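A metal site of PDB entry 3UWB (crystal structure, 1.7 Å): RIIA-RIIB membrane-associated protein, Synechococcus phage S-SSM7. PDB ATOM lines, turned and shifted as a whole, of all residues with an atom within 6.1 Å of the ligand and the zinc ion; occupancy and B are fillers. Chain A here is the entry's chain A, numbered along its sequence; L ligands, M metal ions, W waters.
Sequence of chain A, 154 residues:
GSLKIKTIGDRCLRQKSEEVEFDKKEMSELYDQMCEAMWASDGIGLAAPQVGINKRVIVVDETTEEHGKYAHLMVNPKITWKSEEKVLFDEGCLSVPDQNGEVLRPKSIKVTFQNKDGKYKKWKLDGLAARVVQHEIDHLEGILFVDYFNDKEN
The zinc ion is bound by a ring nitrogen (NE2) of His 135 (2.1 Å), a ring nitrogen (NE2) of His 139 (2.1 Å), an oxygen (O2) of the ligand (2.1 Å), an oxygen (O1) of the ligand (2.2 Å) and the side-chain sulfur (SG) of Cys 93 (2.3 Å).
O of Asp 42 touches C13 of the ligand, at 3.98 Å.
CA of Gly 43 touches O3 of the ligand, at 3.2 Å.
Phe 89 touches the ligand.
Glu 91 touches the ligand.
Arg 131 touches the ligand.
Hydrophobic or aromatic side chains within 4 Å of the ligand: Ile 44, Phe 89, Leu 94, His 135 and His 139.
Within 4 Å of the ligand: Asp 42, Gly 43, Ile 44, Gly 45, Gln 50, Phe 89, Asp 90, Glu 91, Gly 92, Cys 93, Leu 94, Arg 131, His 135, Glu 136 and His 139.
Along chain A the residues within 4 Å of the ligand span positions 42 to 139.
The nearest printed residue that does not touch the ligand is Leu 46 (4.1 Å).
NH1 of Arg 131 lies within salt-bridge range of OE2 of Glu 91.
OG of Ser 95 lies within hydrogen-bond range of NE2 of Gln 50, 3.1 Å away.
The side-chain carboxylate (OE1) of Glu 136 lies within hydrogen-bond range of the backbone NH (N) of Ala 47 (3.4 Å).
The backbone NH (N) of Leu 46 lies within hydrogen-bond range of the side-chain carboxylate (OE2) of Glu 136, 3.3 Å away.
OE2 of Glu 91 lies within salt-bridge range of NE of Arg 105, at 2.9 Å.
NE2 of His 139 lies close to NE2 of Gln 50, 3.4 Å away.
OE1 of Glu 91 is in hydrogen-bond range of ND1 of His 135 (2.8 Å).
The backbone NH (N) of Ser 95 sits close to the side-chain sulfur (SG) of Cys 93 (3.4 Å).
The backbone NH of Ile 44 lies within hydrogen-bond range of an oxygen (O3) of the ligand (2.8 Å).
The side-chain carboxylate (OE2) of Glu 136 lies within hydrogen-bond range of a nitrogen (N1) of the ligand, 2.7 Å away.
The backbone NH (N) of Gly 92 lies within hydrogen-bond range of an oxygen (O4) of the ligand.
The side-chain amide oxygen of Gln 50 lies within hydrogen-bond range of a nitrogen (N1) of the ligand (3.5 Å).
An oxygen (O1) of the ligand lies close to the backbone NH of Leu 94 (2.9 Å).
O of Asp 90 is in hydrogen-bond range of O5 of the ligand (2.6 Å).
O of Gly 92 lies within hydrogen-bond range of N2 of the ligand (3.1 Å).
N1 of the ligand lies within hydrogen-bond range of O of Gly 45 (3.2 Å).
Gln 50 touches the zinc ion.
Of the 24 residues printed, 4 come within 4 Å of the zinc ion.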
ATOM      1  N   SER A  41      -2.645  18.540  26.926  1.00  0.00           N
ATOM      2  CA  SER A  41      -2.371  19.980  26.986  1.00  0.00           C
ATOM      3  C   SER A  41      -3.598  20.794  27.404  1.00  0.00           C
ATOM      4  O   SER A  41      -3.623  22.009  27.202  1.00  0.00           O
ATOM      5  CB  SER A  41      -1.838  20.459  25.635  1.00  0.00           C
ATOM      6  OG  SER A  41      -0.477  20.042  25.474  1.00  0.00           O
ATOM      7  N   ASP A  42      -4.585  20.145  28.037  1.00  0.00           N
ATOM      8  CA  ASP A  42      -5.806  20.827  28.510  1.00  0.00           C
ATOM      9  C   ASP A  42      -6.615  21.584  27.423  1.00  0.00           C
ATOM     10  O   ASP A  42      -7.304  22.594  27.709  1.00  0.00           O
ATOM     11  CB  ASP A  42      -5.473  21.715  29.714  1.00  0.00           C
ATOM     12  CG  ASP A  42      -4.867  20.915  30.869  1.00  0.00           C
ATOM     13  OD1 ASP A  42      -5.334  19.799  31.144  1.00  0.00           O
ATOM     14  OD2 ASP A  42      -3.919  21.406  31.473  1.00  0.00           O
ATOM     15  N   GLY A  43      -6.573  21.062  26.200  1.00  0.00           N
ATOM     16  CA  GLY A  43      -7.302  21.679  25.140  1.00  0.00           C
ATOM     17  C   GLY A  43      -8.699  21.121  25.037  1.00  0.00           C
ATOM     18  O   GLY A  43      -9.042  20.086  25.630  1.00  0.00           O
ATOM     19  N   ILE A  44      -9.526  21.850  24.292  1.00  0.00           N
ATOM     20  CA  ILE A  44     -10.910  21.454  24.076  1.00  0.00           C
ATOM     21  C   ILE A  44     -11.276  21.236  22.616  1.00  0.00           C
ATOM     22  O   ILE A  44     -12.439  20.925  22.286  1.00  0.00           O
ATOM     23  CB  ILE A  44     -11.891  22.457  24.749  1.00  0.00           C
ATOM     24  CG1 ILE A  44     -11.846  23.827  24.137  1.00  0.00           C
ATOM     25  CG2 ILE A  44     -11.677  22.514  26.274  1.00  0.00           C
ATOM     26  CD1 ILE A  44     -13.054  24.687  24.572  1.00  0.00           C
ATOM     27  N   GLY A  45     -10.285  21.395  21.753  1.00  0.00           N
ATOM     28  CA  GLY A  45     -10.367  21.029  20.360  1.00  0.00           C
ATOM     29  C   GLY A  45      -8.954  20.864  19.803  1.00  0.00           C
ATOM     30  O   GLY A  45      -7.956  21.265  20.435  1.00  0.00           O
ATOM     31  N   LEU A  46      -8.850  20.247  18.634  1.00  0.00           N
ATOM     32  CA  LEU A  46      -7.589  20.106  17.930  1.00  0.00           C
ATOM     33  C   LEU A  46      -7.796  19.855  16.461  1.00  0.00           C
ATOM     34  O   LEU A  46      -8.804  19.254  16.090  1.00  0.00           O
ATOM     35  CB  LEU A  46      -6.711  18.972  18.513  1.00  0.00           C
ATOM     36  CG  LEU A  46      -5.178  19.062  18.315  1.00  0.00           C
ATOM     37  CD1 LEU A  46      -4.557  20.170  19.206  1.00  0.00           C
ATOM     38  CD2 LEU A  46      -4.486  17.722  18.644  1.00  0.00           C
ATOM     39  N   ALA A  47      -6.884  20.366  15.633  1.00  0.00           N
ATOM     40  CA  ALA A  47      -6.946  20.187  14.193  1.00  0.00           C
ATOM     41  C   ALA A  47      -5.685  19.480  13.744  1.00  0.00           C
ATOM     42  O   ALA A  47      -4.577  19.782  14.224  1.00  0.00           O
ATOM     43  CB  ALA A  47      -7.105  21.551  13.467  1.00  0.00           C
ATOM     44  N   GLN A  50      -2.195  21.063  13.260  1.00  0.00           N
ATOM     45  CA  GLN A  50      -1.447  21.417  14.472  1.00  0.00           C
ATOM     46  C   GLN A  50      -0.468  20.350  14.921  1.00  0.00           C
ATOM     47  O   GLN A  50       0.435  20.646  15.732  1.00  0.00           O
ATOM     48  CB  GLN A  50      -2.418  21.693  15.637  1.00  0.00           C
ATOM     49  CG  GLN A  50      -3.324  22.902  15.456  1.00  0.00           C
ATOM     50  CD  GLN A  50      -4.193  23.039  16.678  1.00  0.00           C
ATOM     51  OE1 GLN A  50      -5.224  22.369  16.787  1.00  0.00           O
ATOM     52  NE2 GLN A  50      -3.740  23.852  17.660  1.00  0.00           N
ATOM     53  N   PHE A  89     -15.558  36.144  22.296  1.00  0.00           N
ATOM     54  CA  PHE A  89     -15.043  35.109  23.218  1.00  0.00           C
ATOM     55  C   PHE A  89     -13.521  35.130  23.239  1.00  0.00           C
ATOM     56  O   PHE A  89     -12.870  35.339  22.195  1.00  0.00           O
ATOM     57  CB  PHE A  89     -15.592  33.736  22.830  1.00  0.00           C
ATOM     58  CG  PHE A  89     -15.480  32.694  23.920  1.00  0.00           C
ATOM     59  CD1 PHE A  89     -16.424  32.643  24.936  1.00  0.00           C
ATOM     60  CD2 PHE A  89     -14.440  31.797  23.934  1.00  0.00           C
ATOM     61  CE1 PHE A  89     -16.334  31.688  25.944  1.00  0.00           C
ATOM     62  CE2 PHE A  89     -14.349  30.823  24.921  1.00  0.00           C
ATOM     63  CZ  PHE A  89     -15.296  30.785  25.926  1.00  0.00           C
ATOM     64  N   ASP A  90     -12.958  34.962  24.452  1.00  0.00           N
ATOM     65  CA  ASP A  90     -11.523  35.055  24.633  1.00  0.00           C
ATOM     66  C   ASP A  90     -10.894  33.713  24.284  1.00  0.00           C
ATOM     67  O   ASP A  90     -11.237  32.698  24.897  1.00  0.00           O
ATOM     68  CB  ASP A  90     -11.232  35.385  26.120  1.00  0.00           C
ATOM     69  CG  ASP A  90      -9.798  35.805  26.374  1.00  0.00           C
ATOM     70  OD1 ASP A  90      -9.006  36.004  25.453  1.00  0.00           O
ATOM     71  OD2 ASP A  90      -9.432  36.060  27.549  1.00  0.00           O
ATOM     72  N   GLU A  91     -10.045  33.678  23.245  1.00  0.00           N
ATOM     73  CA  GLU A  91      -9.455  32.419  22.797  1.00  0.00           C
ATOM     74  C   GLU A  91      -7.976  32.353  23.089  1.00  0.00           C
ATOM     75  O   GLU A  91      -7.259  33.356  23.039  1.00  0.00           O
ATOM     76  CB  GLU A  91      -9.600  32.270  21.275  1.00  0.00           C
ATOM     77  CG  GLU A  91     -11.024  32.357  20.812  1.00  0.00           C
ATOM     78  CD  GLU A  91     -11.226  32.040  19.366  1.00  0.00           C
ATOM     79  OE1 GLU A  91     -10.316  31.443  18.689  1.00  0.00           O
ATOM     80  OE2 GLU A  91     -12.332  32.333  18.874  1.00  0.00           O
ATOM     81  N   GLY A  92      -7.506  31.125  23.330  1.00  0.00           N
ATOM     82  CA  GLY A  92      -6.110  30.782  23.265  1.00  0.00           C
ATOM     83  C   GLY A  92      -5.979  29.584  22.319  1.00  0.00           C
ATOM     84  O   GLY A  92      -6.983  28.905  21.993  1.00  0.00           O
ATOM     85  N   CYS A  93      -4.763  29.316  21.885  1.00  0.00           N
ATOM     86  CA  CYS A  93      -4.535  28.260  20.918  1.00  0.00           C
ATOM     87  C   CYS A  93      -3.295  27.496  21.362  1.00  0.00           C
ATOM     88  O   CYS A  93      -2.266  28.122  21.729  1.00  0.00           O
ATOM     89  CB  CYS A  93      -4.276  28.853  19.504  1.00  0.00           C
ATOM     90  SG  CYS A  93      -3.959  27.649  18.177  1.00  0.00           S
ATOM     91  N   LEU A  94      -3.365  26.176  21.299  1.00  0.00           N
ATOM     92  CA  LEU A  94      -2.208  25.348  21.672  1.00  0.00           C
ATOM     93  C   LEU A  94      -1.010  25.531  20.711  1.00  0.00           C
ATOM     94  O   LEU A  94       0.098  25.198  21.066  1.00  0.00           O
ATOM     95  CB  LEU A  94      -2.652  23.867  21.775  1.00  0.00           C
ATOM     96  CG  LEU A  94      -3.573  23.582  22.991  1.00  0.00           C
ATOM     97  CD1 LEU A  94      -3.991  22.124  22.881  1.00  0.00           C
ATOM     98  CD2 LEU A  94      -2.887  23.879  24.330  1.00  0.00           C
ATOM     99  N   SER A  95      -1.254  26.077  19.524  1.00  0.00           N
ATOM    100  CA  SER A  95      -0.211  26.385  18.584  1.00  0.00           C
ATOM    101  C   SER A  95       0.303  27.824  18.716  1.00  0.00           C
ATOM    102  O   SER A  95       1.193  28.222  17.945  1.00  0.00           O
ATOM    103  CB  SER A  95      -0.655  26.061  17.160  1.00  0.00           C
ATOM    104  OG  SER A  95      -0.862  24.666  16.975  1.00  0.00           O
ATOM    105  N   ARG A 105     -16.986  35.986  16.400  1.00  0.00           N
ATOM    106  CA  ARG A 105     -17.428  34.968  15.455  1.00  0.00           C
ATOM    107  C   ARG A 105     -18.940  34.776  15.565  1.00  0.00           C
ATOM    108  O   ARG A 105     -19.545  35.033  16.614  1.00  0.00           O
ATOM    109  CB  ARG A 105     -16.763  33.613  15.689  1.00  0.00           C
ATOM    110  CG  ARG A 105     -15.258  33.606  15.832  1.00  0.00           C
ATOM    111  CD  ARG A 105     -14.761  32.177  15.913  1.00  0.00           C
ATOM    112  NE  ARG A 105     -13.344  32.065  16.215  1.00  0.00           N
ATOM    113  CZ  ARG A 105     -12.340  31.813  15.358  1.00  0.00           C
ATOM    114  NH1 ARG A 105     -12.579  31.744  14.047  1.00  0.00           N
ATOM    115  NH2 ARG A 105     -11.129  31.628  15.833  1.00  0.00           N
ATOM    116  N   LEU A 128     -20.224  27.025  23.036  1.00  0.00           N
ATOM    117  CA  LEU A 128     -18.817  26.667  22.987  1.00  0.00           C
ATOM    118  C   LEU A 128     -18.511  25.724  21.803  1.00  0.00           C
ATOM    119  O   LEU A 128     -17.426  25.879  21.143  1.00  0.00           O
ATOM    120  CB  LEU A 128     -18.390  26.037  24.301  1.00  0.00           C
ATOM    121  CG  LEU A 128     -16.879  25.816  24.488  1.00  0.00           C
ATOM    122  CD1 LEU A 128     -16.067  27.110  24.397  1.00  0.00           C
ATOM    123  CD2 LEU A 128     -16.624  25.169  25.838  1.00  0.00           C
ATOM    124  N   ARG A 131     -18.077  27.667  18.720  1.00  0.00           N
ATOM    125  CA  ARG A 131     -16.848  28.397  18.828  1.00  0.00           C
ATOM    126  C   ARG A 131     -15.622  27.556  18.484  1.00  0.00           C
ATOM    127  O   ARG A 131     -14.750  27.959  17.706  1.00  0.00           O
ATOM    128  CB  ARG A 131     -16.746  29.037  20.249  1.00  0.00           C
ATOM    129  CG  ARG A 131     -15.421  29.701  20.560  1.00  0.00           C
ATOM    130  CD  ARG A 131     -15.042  30.785  19.556  1.00  0.00           C
ATOM    131  NE  ARG A 131     -16.094  31.764  19.368  1.00  0.00           N
ATOM    132  CZ  ARG A 131     -15.945  33.086  19.395  1.00  0.00           C
ATOM    133  NH1 ARG A 131     -14.731  33.598  19.540  1.00  0.00           N
ATOM    134  NH2 ARG A 131     -16.998  33.875  19.228  1.00  0.00           N
ATOM    135  N   VAL A 132     -15.527  26.384  19.123  1.00  0.00           N
ATOM    136  CA  VAL A 132     -14.394  25.468  18.948  1.00  0.00           C
ATOM    137  C   VAL A 132     -14.322  25.065  17.492  1.00  0.00           C
ATOM    138  O   VAL A 132     -13.247  25.091  16.902  1.00  0.00           O
ATOM    139  CB  VAL A 132     -14.474  24.245  19.887  1.00  0.00           C
ATOM    140  CG1 VAL A 132     -13.395  23.230  19.492  1.00  0.00           C
ATOM    141  CG2 VAL A 132     -14.381  24.736  21.358  1.00  0.00           C
ATOM    142  N   HIS A 135     -12.832  27.790  15.250  1.00  0.00           N
ATOM    143  CA  HIS A 135     -11.398  27.906  15.516  1.00  0.00           C
ATOM    144  C   HIS A 135     -10.645  26.804  14.806  1.00  0.00           C
ATOM    145  O   HIS A 135      -9.625  27.008  14.155  1.00  0.00           O
ATOM    146  CB  HIS A 135     -11.164  27.925  17.048  1.00  0.00           C
ATOM    147  CG  HIS A 135      -9.720  27.933  17.443  1.00  0.00           C
ATOM    148  ND1 HIS A 135      -9.118  29.020  18.053  1.00  0.00           N
ATOM    149  CD2 HIS A 135      -8.776  26.943  17.393  1.00  0.00           C
ATOM    150  CE1 HIS A 135      -7.830  28.717  18.332  1.00  0.00           C
ATOM    151  NE2 HIS A 135      -7.606  27.463  17.926  1.00  0.00           N
ATOM    152  N   GLU A 136     -11.136  25.575  14.924  1.00  0.00           N
ATOM    153  CA  GLU A 136     -10.481  24.419  14.287  1.00  0.00           C
ATOM    154  C   GLU A 136     -10.554  24.459  12.758  1.00  0.00           C
ATOM    155  O   GLU A 136      -9.543  24.113  12.115  1.00  0.00           O
ATOM    156  CB  GLU A 136     -11.049  23.092  14.792  1.00  0.00           C
ATOM    157  CG  GLU A 136     -11.046  22.863  16.318  1.00  0.00           C
ATOM    158  CD  GLU A 136      -9.743  23.142  17.014  1.00  0.00           C
ATOM    159  OE1 GLU A 136      -8.656  23.129  16.354  1.00  0.00           O
ATOM    160  OE2 GLU A 136      -9.768  23.386  18.254  1.00  0.00           O
ATOM    161  N   HIS A 139      -7.895  26.588  11.380  1.00  0.00           N
ATOM    162  CA  HIS A 139      -6.608  25.906  11.258  1.00  0.00           C
ATOM    163  C   HIS A 139      -6.466  25.178   9.943  1.00  0.00           C
ATOM    164  O   HIS A 139      -5.338  25.146   9.372  1.00  0.00           O
ATOM    165  CB  HIS A 139      -6.396  24.894  12.403  1.00  0.00           C
ATOM    166  CG  HIS A 139      -5.886  25.488  13.659  1.00  0.00           C
ATOM    167  ND1 HIS A 139      -4.696  26.138  13.743  1.00  0.00           N
ATOM    168  CD2 HIS A 139      -6.439  25.500  14.938  1.00  0.00           C
ATOM    169  CE1 HIS A 139      -4.470  26.517  15.017  1.00  0.00           C
ATOM    170  NE2 HIS A 139      -5.522  26.114  15.774  1.00  0.00           N
ATOM    171  N   LEU A 144      -4.605  31.354  12.014  1.00  0.00           N
ATOM    172  CA  LEU A 144      -4.423  31.398  13.432  1.00  0.00           C
ATOM    173  C   LEU A 144      -5.199  32.558  14.038  1.00  0.00           C
ATOM    174  O   LEU A 144      -5.357  33.602  13.399  1.00  0.00           O
ATOM    175  CB  LEU A 144      -2.937  31.489  13.811  1.00  0.00           C
ATOM    176  CG  LEU A 144      -2.005  30.382  13.281  1.00  0.00           C
ATOM    177  CD1 LEU A 144      -0.522  30.623  13.616  1.00  0.00           C
ATOM    178  CD2 LEU A 144      -2.494  28.986  13.718  1.00  0.00           C
ATOM    179  N   PHE A 145      -5.693  32.382  15.265  1.00  0.00           N
ATOM    180  CA  PHE A 145      -6.639  33.369  15.791  1.00  0.00           C
ATOM    181  C   PHE A 145      -6.002  34.742  15.924  1.00  0.00           C
ATOM    182  O   PHE A 145      -6.676  35.748  15.878  1.00  0.00           O
ATOM    183  CB  PHE A 145      -7.246  32.902  17.116  1.00  0.00           C
ATOM    184  CG  PHE A 145      -6.367  33.127  18.310  1.00  0.00           C
ATOM    185  CD1 PHE A 145      -6.529  34.287  19.087  1.00  0.00           C
ATOM    186  CD2 PHE A 145      -5.336  32.234  18.639  1.00  0.00           C
ATOM    187  CE1 PHE A 145      -5.737  34.505  20.178  1.00  0.00           C
ATOM    188  CE2 PHE A 145      -4.521  32.465  19.738  1.00  0.00           C
ATOM    189  CZ  PHE A 145      -4.729  33.611  20.477  1.00  0.00           C
HETATM  190  C1  LIG L   1      -7.094  24.362  21.405  1.00  0.00           C
HETATM  191  C2  LIG L   1      -6.626  24.634  20.021  1.00  0.00           C
HETATM  192  O1  LIG L   1      -5.665  25.367  19.792  1.00  0.00           O
HETATM  193  N1  LIG L   1      -7.285  24.070  18.999  1.00  0.00           N
HETATM  194  O2  LIG L   1      -6.941  24.522  17.720  1.00  0.00           O
HETATM  195  C3  LIG L   1      -8.016  25.504  21.875  1.00  0.00           C
HETATM  196  C4  LIG L   1      -8.162  25.478  23.349  1.00  0.00           C
HETATM  197  O3  LIG L   1      -8.435  24.433  23.955  1.00  0.00           O
HETATM  198  C5  LIG L   1      -9.377  25.426  21.211  1.00  0.00           C
HETATM  199  C6  LIG L   1     -10.376  26.492  21.708  1.00  0.00           C
HETATM  200  C7  LIG L   1     -10.404  27.695  20.870  1.00  0.00           C
HETATM  201  C8  LIG L   1     -11.714  28.539  20.888  1.00  0.00           C
HETATM  202  C9  LIG L   1     -12.162  28.832  22.309  1.00  0.00           C
HETATM  203  N2  LIG L   1      -7.929  26.702  23.935  1.00  0.00           N
HETATM  204  C10 LIG L   1      -8.172  26.917  25.364  1.00  0.00           C
HETATM  205  C11 LIG L   1      -6.837  27.197  26.060  1.00  0.00           C
HETATM  206  C12 LIG L   1      -7.028  27.666  27.507  1.00  0.00           C
HETATM  207  C13 LIG L   1      -5.978  25.922  25.971  1.00  0.00           C
HETATM  208  C14 LIG L   1      -9.148  28.042  25.498  1.00  0.00           C
HETATM  209  O4  LIG L   1      -9.068  29.006  24.772  1.00  0.00           O
HETATM  210  N3  LIG L   1     -10.086  27.991  26.496  1.00  0.00           N
HETATM  211  C15 LIG L   1     -11.239  28.927  26.399  1.00  0.00           C
HETATM  212  C16 LIG L   1     -10.516  26.665  27.016  1.00  0.00           C
HETATM  213  C17 LIG L   1     -11.844  26.968  27.740  1.00  0.00           C
HETATM  214  C18 LIG L   1     -12.427  28.179  27.015  1.00  0.00           C
HETATM  215  C19 LIG L   1     -10.913  30.189  27.198  1.00  0.00           C
HETATM  216  O5  LIG L   1     -11.804  31.335  26.980  1.00  0.00           O
HETATM  217 ZN    ZN M   1      -5.854  26.366  17.839  1.00  0.00          ZN
HETATM  218  O   HOH W   1      -8.702  24.525  28.732  1.00  0.00           O
